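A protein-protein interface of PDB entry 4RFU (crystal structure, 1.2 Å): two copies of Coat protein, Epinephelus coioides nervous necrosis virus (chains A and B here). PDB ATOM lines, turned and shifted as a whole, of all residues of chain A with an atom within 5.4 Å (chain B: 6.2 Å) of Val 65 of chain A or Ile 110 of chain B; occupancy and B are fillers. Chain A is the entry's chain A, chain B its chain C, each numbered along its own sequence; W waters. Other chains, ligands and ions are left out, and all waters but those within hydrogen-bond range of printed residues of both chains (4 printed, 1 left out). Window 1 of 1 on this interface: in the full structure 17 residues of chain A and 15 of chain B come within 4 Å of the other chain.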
ATOM      1  N   PRO A  49     -13.715 -16.668 -21.890  1.00  0.00           N
ATOM      2  CA  PRO A  49     -13.115 -17.636 -20.968  1.00  0.00           C
ATOM      3  C   PRO A  49     -11.660 -17.933 -21.286  1.00  0.00           C
ATOM      4  O   PRO A  49     -11.295 -18.057 -22.453  1.00  0.00           O
ATOM      5  CB  PRO A  49     -13.960 -18.896 -21.195  1.00  0.00           C
ATOM      6  CG  PRO A  49     -14.459 -18.763 -22.596  1.00  0.00           C
ATOM      7  CD  PRO A  49     -14.701 -17.294 -22.792  1.00  0.00           C
ATOM      8  N   LEU A  50     -10.848 -18.042 -20.239  1.00  0.00           N
ATOM      9  CA  LEU A  50      -9.494 -18.534 -20.353  1.00  0.00           C
ATOM     10  C   LEU A  50      -9.457 -19.984 -19.898  1.00  0.00           C
ATOM     11  O   LEU A  50      -9.581 -20.275 -18.708  1.00  0.00           O
ATOM     12  CB  LEU A  50      -8.557 -17.689 -19.500  1.00  0.00           C
ATOM     13  CG  LEU A  50      -7.118 -18.177 -19.361  1.00  0.00           C
ATOM     14  CD1 LEU A  50      -6.461 -18.456 -20.709  1.00  0.00           C
ATOM     15  CD2 LEU A  50      -6.297 -17.181 -18.529  1.00  0.00           C
ATOM     16  N   SER A  51      -9.322 -20.898 -20.844  1.00  0.00           N
ATOM     17  CA  SER A  51      -9.269 -22.314 -20.510  1.00  0.00           C
ATOM     18  C   SER A  51      -7.852 -22.753 -20.226  1.00  0.00           C
ATOM     19  O   SER A  51      -6.930 -22.456 -20.981  1.00  0.00           O
ATOM     20  CB  SER A  51      -9.872 -23.174 -21.614  1.00  0.00           C
ATOM     21  OG  SER A  51     -11.284 -23.095 -21.575  1.00  0.00           O
ATOM     22  N   ILE A  52      -7.702 -23.464 -19.122  1.00  0.00           N
ATOM     23  CA  ILE A  52      -6.416 -23.927 -18.643  1.00  0.00           C
ATOM     24  C   ILE A  52      -6.452 -25.446 -18.507  1.00  0.00           C
ATOM     25  O   ILE A  52      -7.162 -25.990 -17.647  1.00  0.00           O
ATOM     26  CB  ILE A  52      -6.088 -23.289 -17.271  1.00  0.00           C
ATOM     27  CG1 ILE A  52      -5.989 -21.762 -17.399  1.00  0.00           C
ATOM     28  CG2 ILE A  52      -4.815 -23.894 -16.670  1.00  0.00           C
ATOM     29  CD1 ILE A  52      -4.827 -21.272 -18.240  1.00  0.00           C
ATOM     30  N   ARG A  63      -9.533 -30.091 -18.194  1.00  0.00           N
ATOM     31  CA  ARG A  63      -9.649 -28.683 -18.577  1.00  0.00           C
ATOM     32  C   ARG A  63     -10.464 -27.861 -17.583  1.00  0.00           C
ATOM     33  O   ARG A  63     -11.558 -28.271 -17.165  1.00  0.00           O
ATOM     34  CB  ARG A  63     -10.219 -28.554 -19.999  1.00  0.00           C
ATOM     35  CG  ARG A  63     -10.376 -27.121 -20.498  1.00  0.00           C
ATOM     36  CD  ARG A  63     -10.419 -27.026 -22.011  1.00  0.00           C
ATOM     37  NE  ARG A  63      -9.064 -26.879 -22.521  1.00  0.00           N
ATOM     38  CZ  ARG A  63      -8.715 -26.196 -23.606  1.00  0.00           C
ATOM     39  NH1 ARG A  63      -9.605 -25.565 -24.370  1.00  0.00           N
ATOM     40  NH2 ARG A  63      -7.441 -26.158 -23.948  1.00  0.00           N
ATOM     41  N   ALA A  64      -9.909 -26.713 -17.195  1.00  0.00           N
ATOM     42  CA  ALA A  64     -10.553 -25.773 -16.279  1.00  0.00           C
ATOM     43  C   ALA A  64     -10.860 -24.460 -17.004  1.00  0.00           C
ATOM     44  O   ALA A  64     -10.264 -24.162 -18.041  1.00  0.00           O
ATOM     45  CB  ALA A  64      -9.656 -25.500 -15.082  1.00  0.00           C
ATOM     46  N   VAL A  65     -11.759 -23.657 -16.438  1.00  0.00           N
ATOM     47  CA  VAL A  65     -12.051 -22.323 -16.965  1.00  0.00           C
ATOM     48  C   VAL A  65     -11.817 -21.252 -15.904  1.00  0.00           C
ATOM     49  O   VAL A  65     -12.157 -21.444 -14.730  1.00  0.00           O
ATOM     50  CB  VAL A  65     -13.498 -22.217 -17.538  1.00  0.00           C
ATOM     51  CG1 VAL A  65     -14.556 -22.454 -16.453  1.00  0.00           C
ATOM     52  CG2 VAL A  65     -13.718 -20.872 -18.222  1.00  0.00           C
ATOM     53  N   TYR A  66     -11.226 -20.135 -16.341  1.00  0.00           N
ATOM     54  CA  TYR A  66     -11.010 -18.958 -15.510  1.00  0.00           C
ATOM     55  C   TYR A  66     -11.474 -17.698 -16.228  1.00  0.00           C
ATOM     56  O   TYR A  66     -11.437 -17.612 -17.456  1.00  0.00           O
ATOM     57  CB  TYR A  66      -9.531 -18.846 -15.099  1.00  0.00           C
ATOM     58  CG  TYR A  66      -9.152 -20.001 -14.214  1.00  0.00           C
ATOM     59  CD1 TYR A  66      -9.467 -19.982 -12.864  1.00  0.00           C
ATOM     60  CD2 TYR A  66      -8.541 -21.135 -14.730  1.00  0.00           C
ATOM     61  CE1 TYR A  66      -9.178 -21.051 -12.046  1.00  0.00           C
ATOM     62  CE2 TYR A  66      -8.249 -22.219 -13.914  1.00  0.00           C
ATOM     63  CZ  TYR A  66      -8.569 -22.169 -12.578  1.00  0.00           C
ATOM     64  OH  TYR A  66      -8.266 -23.243 -11.775  1.00  0.00           O
ATOM     65  N   TRP A  67     -11.900 -16.715 -15.440  1.00  0.00           N
ATOM     66  CA  TRP A  67     -12.399 -15.450 -15.967  1.00  0.00           C
ATOM     67  C   TRP A  67     -11.654 -14.255 -15.397  1.00  0.00           C
ATOM     68  O   TRP A  67     -11.993 -13.115 -15.726  1.00  0.00           O
ATOM     69  CB  TRP A  67     -13.890 -15.289 -15.661  1.00  0.00           C
ATOM     70  CG  TRP A  67     -14.737 -16.403 -16.171  1.00  0.00           C
ATOM     71  CD1 TRP A  67     -15.084 -17.541 -15.502  1.00  0.00           C
ATOM     72  CD2 TRP A  67     -15.355 -16.484 -17.456  1.00  0.00           C
ATOM     73  NE1 TRP A  67     -15.879 -18.325 -16.295  1.00  0.00           N
ATOM     74  CE2 TRP A  67     -16.065 -17.701 -17.498  1.00  0.00           C
ATOM     75  CE3 TRP A  67     -15.390 -15.643 -18.573  1.00  0.00           C
ATOM     76  CZ2 TRP A  67     -16.795 -18.101 -18.615  1.00  0.00           C
ATOM     77  CZ3 TRP A  67     -16.115 -16.044 -19.681  1.00  0.00           C
ATOM     78  CH2 TRP A  67     -16.803 -17.263 -19.692  1.00  0.00           C
ATOM     79  N   HIS A  68     -10.664 -14.509 -14.546  1.00  0.00           N
ATOM     80  CA  HIS A  68      -9.985 -13.445 -13.816  1.00  0.00           C
ATOM     81  C   HIS A  68      -8.475 -13.581 -13.862  1.00  0.00           C
ATOM     82  O   HIS A  68      -7.933 -14.689 -13.838  1.00  0.00           O
ATOM     83  CB  HIS A  68     -10.470 -13.398 -12.365  1.00  0.00           C
ATOM     84  CG  HIS A  68     -11.938 -13.166 -12.250  1.00  0.00           C
ATOM     85  ND1 HIS A  68     -12.840 -14.163 -11.933  1.00  0.00           N
ATOM     86  CD2 HIS A  68     -12.670 -12.044 -12.448  1.00  0.00           C
ATOM     87  CE1 HIS A  68     -14.061 -13.660 -11.937  1.00  0.00           C
ATOM     88  NE2 HIS A  68     -13.987 -12.379 -12.248  1.00  0.00           N
ATOM     89  N   ILE A  87      -9.511 -17.012  -9.501  1.00  0.00           N
ATOM     90  CA  ILE A  87     -10.883 -16.698  -9.151  1.00  0.00           C
ATOM     91  C   ILE A  87     -10.949 -15.401  -8.353  1.00  0.00           C
ATOM     92  O   ILE A  87     -10.258 -15.249  -7.338  1.00  0.00           O
ATOM     93  CB  ILE A  87     -11.488 -17.833  -8.293  1.00  0.00           C
ATOM     94  CG1 ILE A  87     -11.750 -19.067  -9.152  1.00  0.00           C
ATOM     95  CG2 ILE A  87     -12.756 -17.379  -7.584  1.00  0.00           C
ATOM     96  CD1 ILE A  87     -12.349 -20.217  -8.375  1.00  0.00           C
ATOM     97  N   TRP A  88     -11.785 -14.477  -8.812  1.00  0.00           N
ATOM     98  CA  TRP A  88     -12.105 -13.279  -8.047  1.00  0.00           C
ATOM     99  C   TRP A  88     -13.457 -13.442  -7.372  1.00  0.00           C
ATOM    100  O   TRP A  88     -14.472 -13.669  -8.032  1.00  0.00           O
ATOM    101  CB  TRP A  88     -12.135 -12.062  -8.961  1.00  0.00           C
ATOM    102  CG  TRP A  88     -12.588 -10.798  -8.296  1.00  0.00           C
ATOM    103  CD1 TRP A  88     -13.759 -10.130  -8.514  1.00  0.00           C
ATOM    104  CD2 TRP A  88     -11.869 -10.043  -7.319  1.00  0.00           C
ATOM    105  NE1 TRP A  88     -13.810  -9.000  -7.729  1.00  0.00           N
ATOM    106  CE2 TRP A  88     -12.662  -8.926  -6.986  1.00  0.00           C
ATOM    107  CE3 TRP A  88     -10.634 -10.204  -6.689  1.00  0.00           C
ATOM    108  CZ2 TRP A  88     -12.259  -7.976  -6.052  1.00  0.00           C
ATOM    109  CZ3 TRP A  88     -10.230  -9.256  -5.762  1.00  0.00           C
ATOM    110  CH2 TRP A  88     -11.043  -8.157  -5.454  1.00  0.00           C
ATOM    111  N   SER B  14     -21.620 -15.148  -8.980  1.00  0.00           N
ATOM    112  CA  SER B  14     -20.910 -16.154  -9.765  1.00  0.00           C
ATOM    113  C   SER B  14     -21.467 -17.544  -9.538  1.00  0.00           C
ATOM    114  O   SER B  14     -21.827 -17.896  -8.419  1.00  0.00           O
ATOM    115  CB  SER B  14     -19.432 -16.162  -9.393  1.00  0.00           C
ATOM    116  OG  SER B  14     -18.810 -14.963  -9.801  1.00  0.00           O
ATOM    117  N   LEU B  15     -21.525 -18.332 -10.601  1.00  0.00           N
ATOM    118  CA  LEU B  15     -21.871 -19.739 -10.482  1.00  0.00           C
ATOM    119  C   LEU B  15     -20.584 -20.548 -10.392  1.00  0.00           C
ATOM    120  O   LEU B  15     -19.798 -20.566 -11.343  1.00  0.00           O
ATOM    121  CB  LEU B  15     -22.683 -20.188 -11.692  1.00  0.00           C
ATOM    122  CG  LEU B  15     -23.126 -21.650 -11.659  1.00  0.00           C
ATOM    123  CD1 LEU B  15     -24.050 -21.916 -10.469  1.00  0.00           C
ATOM    124  CD2 LEU B  15     -23.800 -22.018 -12.966  1.00  0.00           C
ATOM    125  N   TYR B  16     -20.372 -21.200  -9.253  1.00  0.00           N
ATOM    126  CA  TYR B  16     -19.199 -22.036  -9.025  1.00  0.00           C
ATOM    127  C   TYR B  16     -19.517 -23.497  -9.304  1.00  0.00           C
ATOM    128  O   TYR B  16     -20.644 -23.964  -9.056  1.00  0.00           O
ATOM    129  CB  TYR B  16     -18.732 -21.922  -7.576  1.00  0.00           C
ATOM    130  CG  TYR B  16     -18.112 -20.597  -7.215  1.00  0.00           C
ATOM    131  CD1 TYR B  16     -18.889 -19.539  -6.766  1.00  0.00           C
ATOM    132  CD2 TYR B  16     -16.738 -20.408  -7.308  1.00  0.00           C
ATOM    133  CE1 TYR B  16     -18.310 -18.325  -6.421  1.00  0.00           C
ATOM    134  CE2 TYR B  16     -16.156 -19.199  -6.961  1.00  0.00           C
ATOM    135  CZ  TYR B  16     -16.947 -18.166  -6.528  1.00  0.00           C
ATOM    136  OH  TYR B  16     -16.357 -16.965  -6.185  1.00  0.00           O
ATOM    137  N   ASN B  17     -18.517 -24.233  -9.783  1.00  0.00           N
ATOM    138  CA  ASN B  17     -18.712 -25.647 -10.063  1.00  0.00           C
ATOM    139  C   ASN B  17     -19.120 -26.441  -8.830  1.00  0.00           C
ATOM    140  O   ASN B  17     -19.877 -27.410  -8.941  1.00  0.00           O
ATOM    141  CB  ASN B  17     -17.517 -26.287 -10.793  1.00  0.00           C
ATOM    142  CG  ASN B  17     -16.195 -26.156 -10.045  1.00  0.00           C
ATOM    143  OD1 ASN B  17     -16.085 -25.465  -9.031  1.00  0.00           O
ATOM    144  ND2 ASN B  17     -15.166 -26.806 -10.574  1.00  0.00           N
ATOM    145  N   SER B  51     -19.592 -24.408 -19.019  1.00  0.00           N
ATOM    146  CA  SER B  51     -18.865 -25.668 -19.135  1.00  0.00           C
ATOM    147  C   SER B  51     -19.289 -26.635 -18.049  1.00  0.00           C
ATOM    148  O   SER B  51     -19.226 -26.309 -16.864  1.00  0.00           O
ATOM    149  CB  SER B  51     -17.357 -25.439 -19.047  1.00  0.00           C
ATOM    150  OG  SER B  51     -16.840 -25.044 -20.309  1.00  0.00           O
ATOM    151  N   ARG B  63     -15.347 -32.533 -20.779  1.00  0.00           N
ATOM    152  CA  ARG B  63     -16.046 -31.260 -20.656  1.00  0.00           C
ATOM    153  C   ARG B  63     -17.019 -31.052 -21.806  1.00  0.00           C
ATOM    154  O   ARG B  63     -16.665 -31.253 -22.969  1.00  0.00           O
ATOM    155  CB  ARG B  63     -15.033 -30.109 -20.561  1.00  0.00           C
ATOM    156  CG  ARG B  63     -15.634 -28.715 -20.517  1.00  0.00           C
ATOM    157  CD  ARG B  63     -14.713 -27.734 -19.804  1.00  0.00           C
ATOM    158  NE  ARG B  63     -14.818 -27.878 -18.357  1.00  0.00           N
ATOM    159  CZ  ARG B  63     -14.426 -26.965 -17.472  1.00  0.00           C
ATOM    160  NH1 ARG B  63     -13.887 -25.824 -17.886  1.00  0.00           N
ATOM    161  NH2 ARG B  63     -14.584 -27.187 -16.173  1.00  0.00           N
ATOM    162  N   ARG B 108     -11.677 -25.743  -7.922  1.00  0.00           N
ATOM    163  CA  ARG B 108     -12.821 -24.853  -7.866  1.00  0.00           C
ATOM    164  C   ARG B 108     -12.746 -23.870  -9.027  1.00  0.00           C
ATOM    165  O   ARG B 108     -11.674 -23.351  -9.346  1.00  0.00           O
ATOM    166  CB  ARG B 108     -12.826 -24.108  -6.534  1.00  0.00           C
ATOM    167  CG  ARG B 108     -14.074 -23.289  -6.279  1.00  0.00           C
ATOM    168  CD  ARG B 108     -14.192 -22.968  -4.794  1.00  0.00           C
ATOM    169  NE  ARG B 108     -15.469 -22.344  -4.464  1.00  0.00           N
ATOM    170  CZ  ARG B 108     -15.603 -21.066  -4.135  1.00  0.00           C
ATOM    171  NH1 ARG B 108     -14.536 -20.280  -4.084  1.00  0.00           N
ATOM    172  NH2 ARG B 108     -16.802 -20.573  -3.851  1.00  0.00           N
ATOM    173  N   GLN B 109     -13.881 -23.618  -9.667  1.00  0.00           N
ATOM    174  CA  GLN B 109     -13.941 -22.751 -10.841  1.00  0.00           C
ATOM    175  C   GLN B 109     -15.215 -21.946 -10.827  1.00  0.00           C
ATOM    176  O   GLN B 109     -16.261 -22.452 -10.426  1.00  0.00           O
ATOM    177  CB  GLN B 109     -13.924 -23.590 -12.124  1.00  0.00           C
ATOM    178  CG  GLN B 109     -12.625 -24.330 -12.354  1.00  0.00           C
ATOM    179  CD  GLN B 109     -12.791 -25.484 -13.319  1.00  0.00           C
ATOM    180  OE1 GLN B 109     -13.179 -25.289 -14.471  1.00  0.00           O
ATOM    181  NE2 GLN B 109     -12.507 -26.700 -12.852  1.00  0.00           N
ATOM    182  N   ILE B 110     -15.130 -20.702 -11.284  1.00  0.00           N
ATOM    183  CA  ILE B 110     -16.304 -19.940 -11.640  1.00  0.00           C
ATOM    184  C   ILE B 110     -16.681 -20.362 -13.050  1.00  0.00           C
ATOM    185  O   ILE B 110     -15.947 -20.120 -14.008  1.00  0.00           O
ATOM    186  CB  ILE B 110     -16.038 -18.426 -11.596  1.00  0.00           C
ATOM    187  CG1 ILE B 110     -15.842 -17.965 -10.152  1.00  0.00           C
ATOM    188  CG2 ILE B 110     -17.181 -17.672 -12.259  1.00  0.00           C
ATOM    189  CD1 ILE B 110     -15.383 -16.514 -10.040  1.00  0.00           C
ATOM    190  N   LEU B 111     -17.819 -21.027 -13.174  1.00  0.00           N
ATOM    191  CA  LEU B 111     -18.299 -21.450 -14.478  1.00  0.00           C
ATOM    192  C   LEU B 111     -18.932 -20.282 -15.231  1.00  0.00           C
ATOM    193  O   LEU B 111     -18.673 -20.096 -16.420  1.00  0.00           O
ATOM    194  CB  LEU B 111     -19.272 -22.620 -14.340  1.00  0.00           C
ATOM    195  CG  LEU B 111     -18.678 -23.861 -13.678  1.00  0.00           C
ATOM    196  CD1 LEU B 111     -19.727 -24.950 -13.592  1.00  0.00           C
ATOM    197  CD2 LEU B 111     -17.447 -24.355 -14.422  1.00  0.00           C
ATOM    198  N   LEU B 112     -19.744 -19.487 -14.536  1.00  0.00           N
ATOM    199  CA  LEU B 112     -20.327 -18.278 -15.127  1.00  0.00           C
ATOM    200  C   LEU B 112     -20.088 -17.092 -14.214  1.00  0.00           C
ATOM    201  O   LEU B 112     -20.560 -17.094 -13.074  1.00  0.00           O
ATOM    202  CB  LEU B 112     -21.830 -18.438 -15.341  1.00  0.00           C
ATOM    203  CG  LEU B 112     -22.296 -19.466 -16.369  1.00  0.00           C
ATOM    204  CD1 LEU B 112     -23.808 -19.596 -16.322  1.00  0.00           C
ATOM    205  CD2 LEU B 112     -21.846 -19.087 -17.771  1.00  0.00           C
ATOM    206  N   PRO B 113     -19.344 -16.079 -14.696  1.00  0.00           N
ATOM    207  CA  PRO B 113     -19.011 -14.967 -13.810  1.00  0.00           C
ATOM    208  C   PRO B 113     -20.126 -13.937 -13.739  1.00  0.00           C
ATOM    209  O   PRO B 113     -21.061 -13.945 -14.545  1.00  0.00           O
ATOM    210  CB  PRO B 113     -17.778 -14.357 -14.481  1.00  0.00           C
ATOM    211  CG  PRO B 113     -18.033 -14.568 -15.917  1.00  0.00           C
ATOM    212  CD  PRO B 113     -18.721 -15.919 -16.024  1.00  0.00           C
ATOM    213  N   VAL B 114     -20.001 -13.055 -12.757  1.00  0.00           N
ATOM    214  CA  VAL B 114     -20.884 -11.908 -12.622  1.00  0.00           C
ATOM    215  C   VAL B 114     -20.909 -11.130 -13.931  1.00  0.00           C
ATOM    216  O   VAL B 114     -19.862 -10.903 -14.551  1.00  0.00           O
ATOM    217  CB  VAL B 114     -20.416 -10.996 -11.470  1.00  0.00           C
ATOM    218  CG1 VAL B 114     -21.244  -9.718 -11.423  1.00  0.00           C
ATOM    219  CG2 VAL B 114     -20.505 -11.742 -10.143  1.00  0.00           C
HETATM  220  O   HOH W   1     -12.420 -29.146 -14.654  1.00  0.00           O
HETATM  221  O   HOH W   2      -9.023 -23.030  -9.248  1.00  0.00           O
HETATM  222  O   HOH W   3     -13.123 -24.807 -20.373  1.00  0.00           O
HETATM  223  O   HOH W   4     -12.719 -19.915 -12.404  1.00  0.00           O
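Arg 63 of chain B touches its own counterpart, Arg 63 of chain A. 2 positions are printed for both chains. Of the 15 pairs that touch across the chains among the printed residues, 1 has its exchanged pair printed and touching as well.
Printed residues of chain A that touch a printed residue of chain B: Arg 63, Ala 64, Val 65, Trp 67, His 68, Ile 87 and Trp 88. Hydrophobic or aromatic side chains of chain B within 4 Å of the printed part of chain A: Tyr 16, Ile 110 and Pro 113. Among the printed residues, 15 pairs touch across the chains. Among the printed residues, no Asp or Glu carboxylate lies within 4 Å of a Lys or Arg side-chain nitrogen of the other chain.
The backbone NH (N) of Ile 52 of chain A lies within hydrogen-bond range of the backbone carbonyl oxygen (O) of Ala 64 of chain A, 2.9 Å away. A ring nitrogen (ND1) of His 68 of chain A sits at hydrogen-bond distance from the backbone NH (N) of Trp 88 of chain A (3.3 Å). The backbone carbonyl oxygen (O) of Leu 15 of chain B sits at hydrogen-bond distance from the backbone NH (N) of Leu 111 of chain B, at 2.7 Å. N of Asn 17 of chain B is in hydrogen-bond range of O of Gln 109 of chain B. NH2 of Arg 63 of chain B sits at hydrogen-bond distance from OE1 of Gln 109 of chain B (2.9 Å).
Printed residues of chain B within 4 Å of Val 65 of chain A: Arg 63 (3.4 Å), Gln 109 (2.9 Å) and Ile 110 (3.7 Å). Of chain A, only Val 65, Trp 67, His 68, Ile 87 and Trp 88 come within 4 Å of Ile 110 of chain B. Printed residues of chain B within 4 Å of His 68 of chain A: Ile 110. Printed residues of chain A within 4 Å of Leu 111 of chain B: Trp 67. Printed residues of chain A within 4 Å of Arg 63 of chain B: Arg 63 (3.2 Å), Ala 64 (3.4 Å) and Val 65 (3.4 Å). Val 114 of chain B touches none of the printed residues of chain A. Tyr 66 of chain A touches none of the printed residues of chain B. The nearest residue of chain A that does not touch Ile 110 of chain B is Tyr 66 of chain A (5.3 Å). The nearest printed residue of chain B that does not touch Arg 63 of chain A is Gln 109 of chain B (4.3 Å).
Among the printed residues, pairs that only touch across the chains: Ala 64 of chain A with Arg 63 of chain B, Ala 64 of chain A with Gln 109 of chain B, Val 65 of chain A with Ile 110 of chain B, Trp 67 of chain A with Pro 113 of chain B, His 68 of chain A with Ile 110 of chain B, Ile 87 of chain A with Tyr 16 of chain B, Ile 87 of chain A with Arg 108 of chain B, Ile 87 of chain A with Gln 109 of chain B, Ile 87 of chain A with Ile 110 of chain B and Trp 88 of chain A with Ile 110 of chain B.
Water W2 lies within hydrogen-bond range of the side-chain hydroxyl of Tyr 66 of chain A (2.6 Å) and the backbone carbonyl oxygen of Arg 108 of chain B (2.7 Å). Water W4 lies within hydrogen-bond range of the backbone NH of Ile 110 of chain B and the backbone carbonyl oxygen of Val 65 of chain A. Water W3 lies within hydrogen-bond range of OG of Ser 51 of chain A (2.8 Å) and NH1 of Arg 63 of chain B (2.8 Å). Water W1 lies within hydrogen-bond range of the backbone carbonyl oxygen of Arg 63 of chain A (2.8 Å), the side-chain amide nitrogen of Gln 109 of chain B (3.0 Å) and the guanidinium group of Arg 63 of chain B (3.3 Å).
The backbone carbonyl oxygen of Arg 63 of chain A sits close to the guanidinium group of Arg 63 of chain B (3.4 Å). N of Val 65 of chain A sits at hydrogen-bond distance from OE1 of Gln 109 of chain B, at 2.9 Å. NE1 of Trp 67 of chain A sits at hydrogen-bond distance from O of Ile 110 of chain B. The indole nitrogen of Trp 67 of chain A sits at hydrogen-bond distance from the backbone carbonyl oxygen of Leu 111 of chain B, at 3.3 Å. The backbone NH (N) of Val 65 of chain A lies close to the guanidinium group (NH1) of Arg 63 of chain B (3.4 Å).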
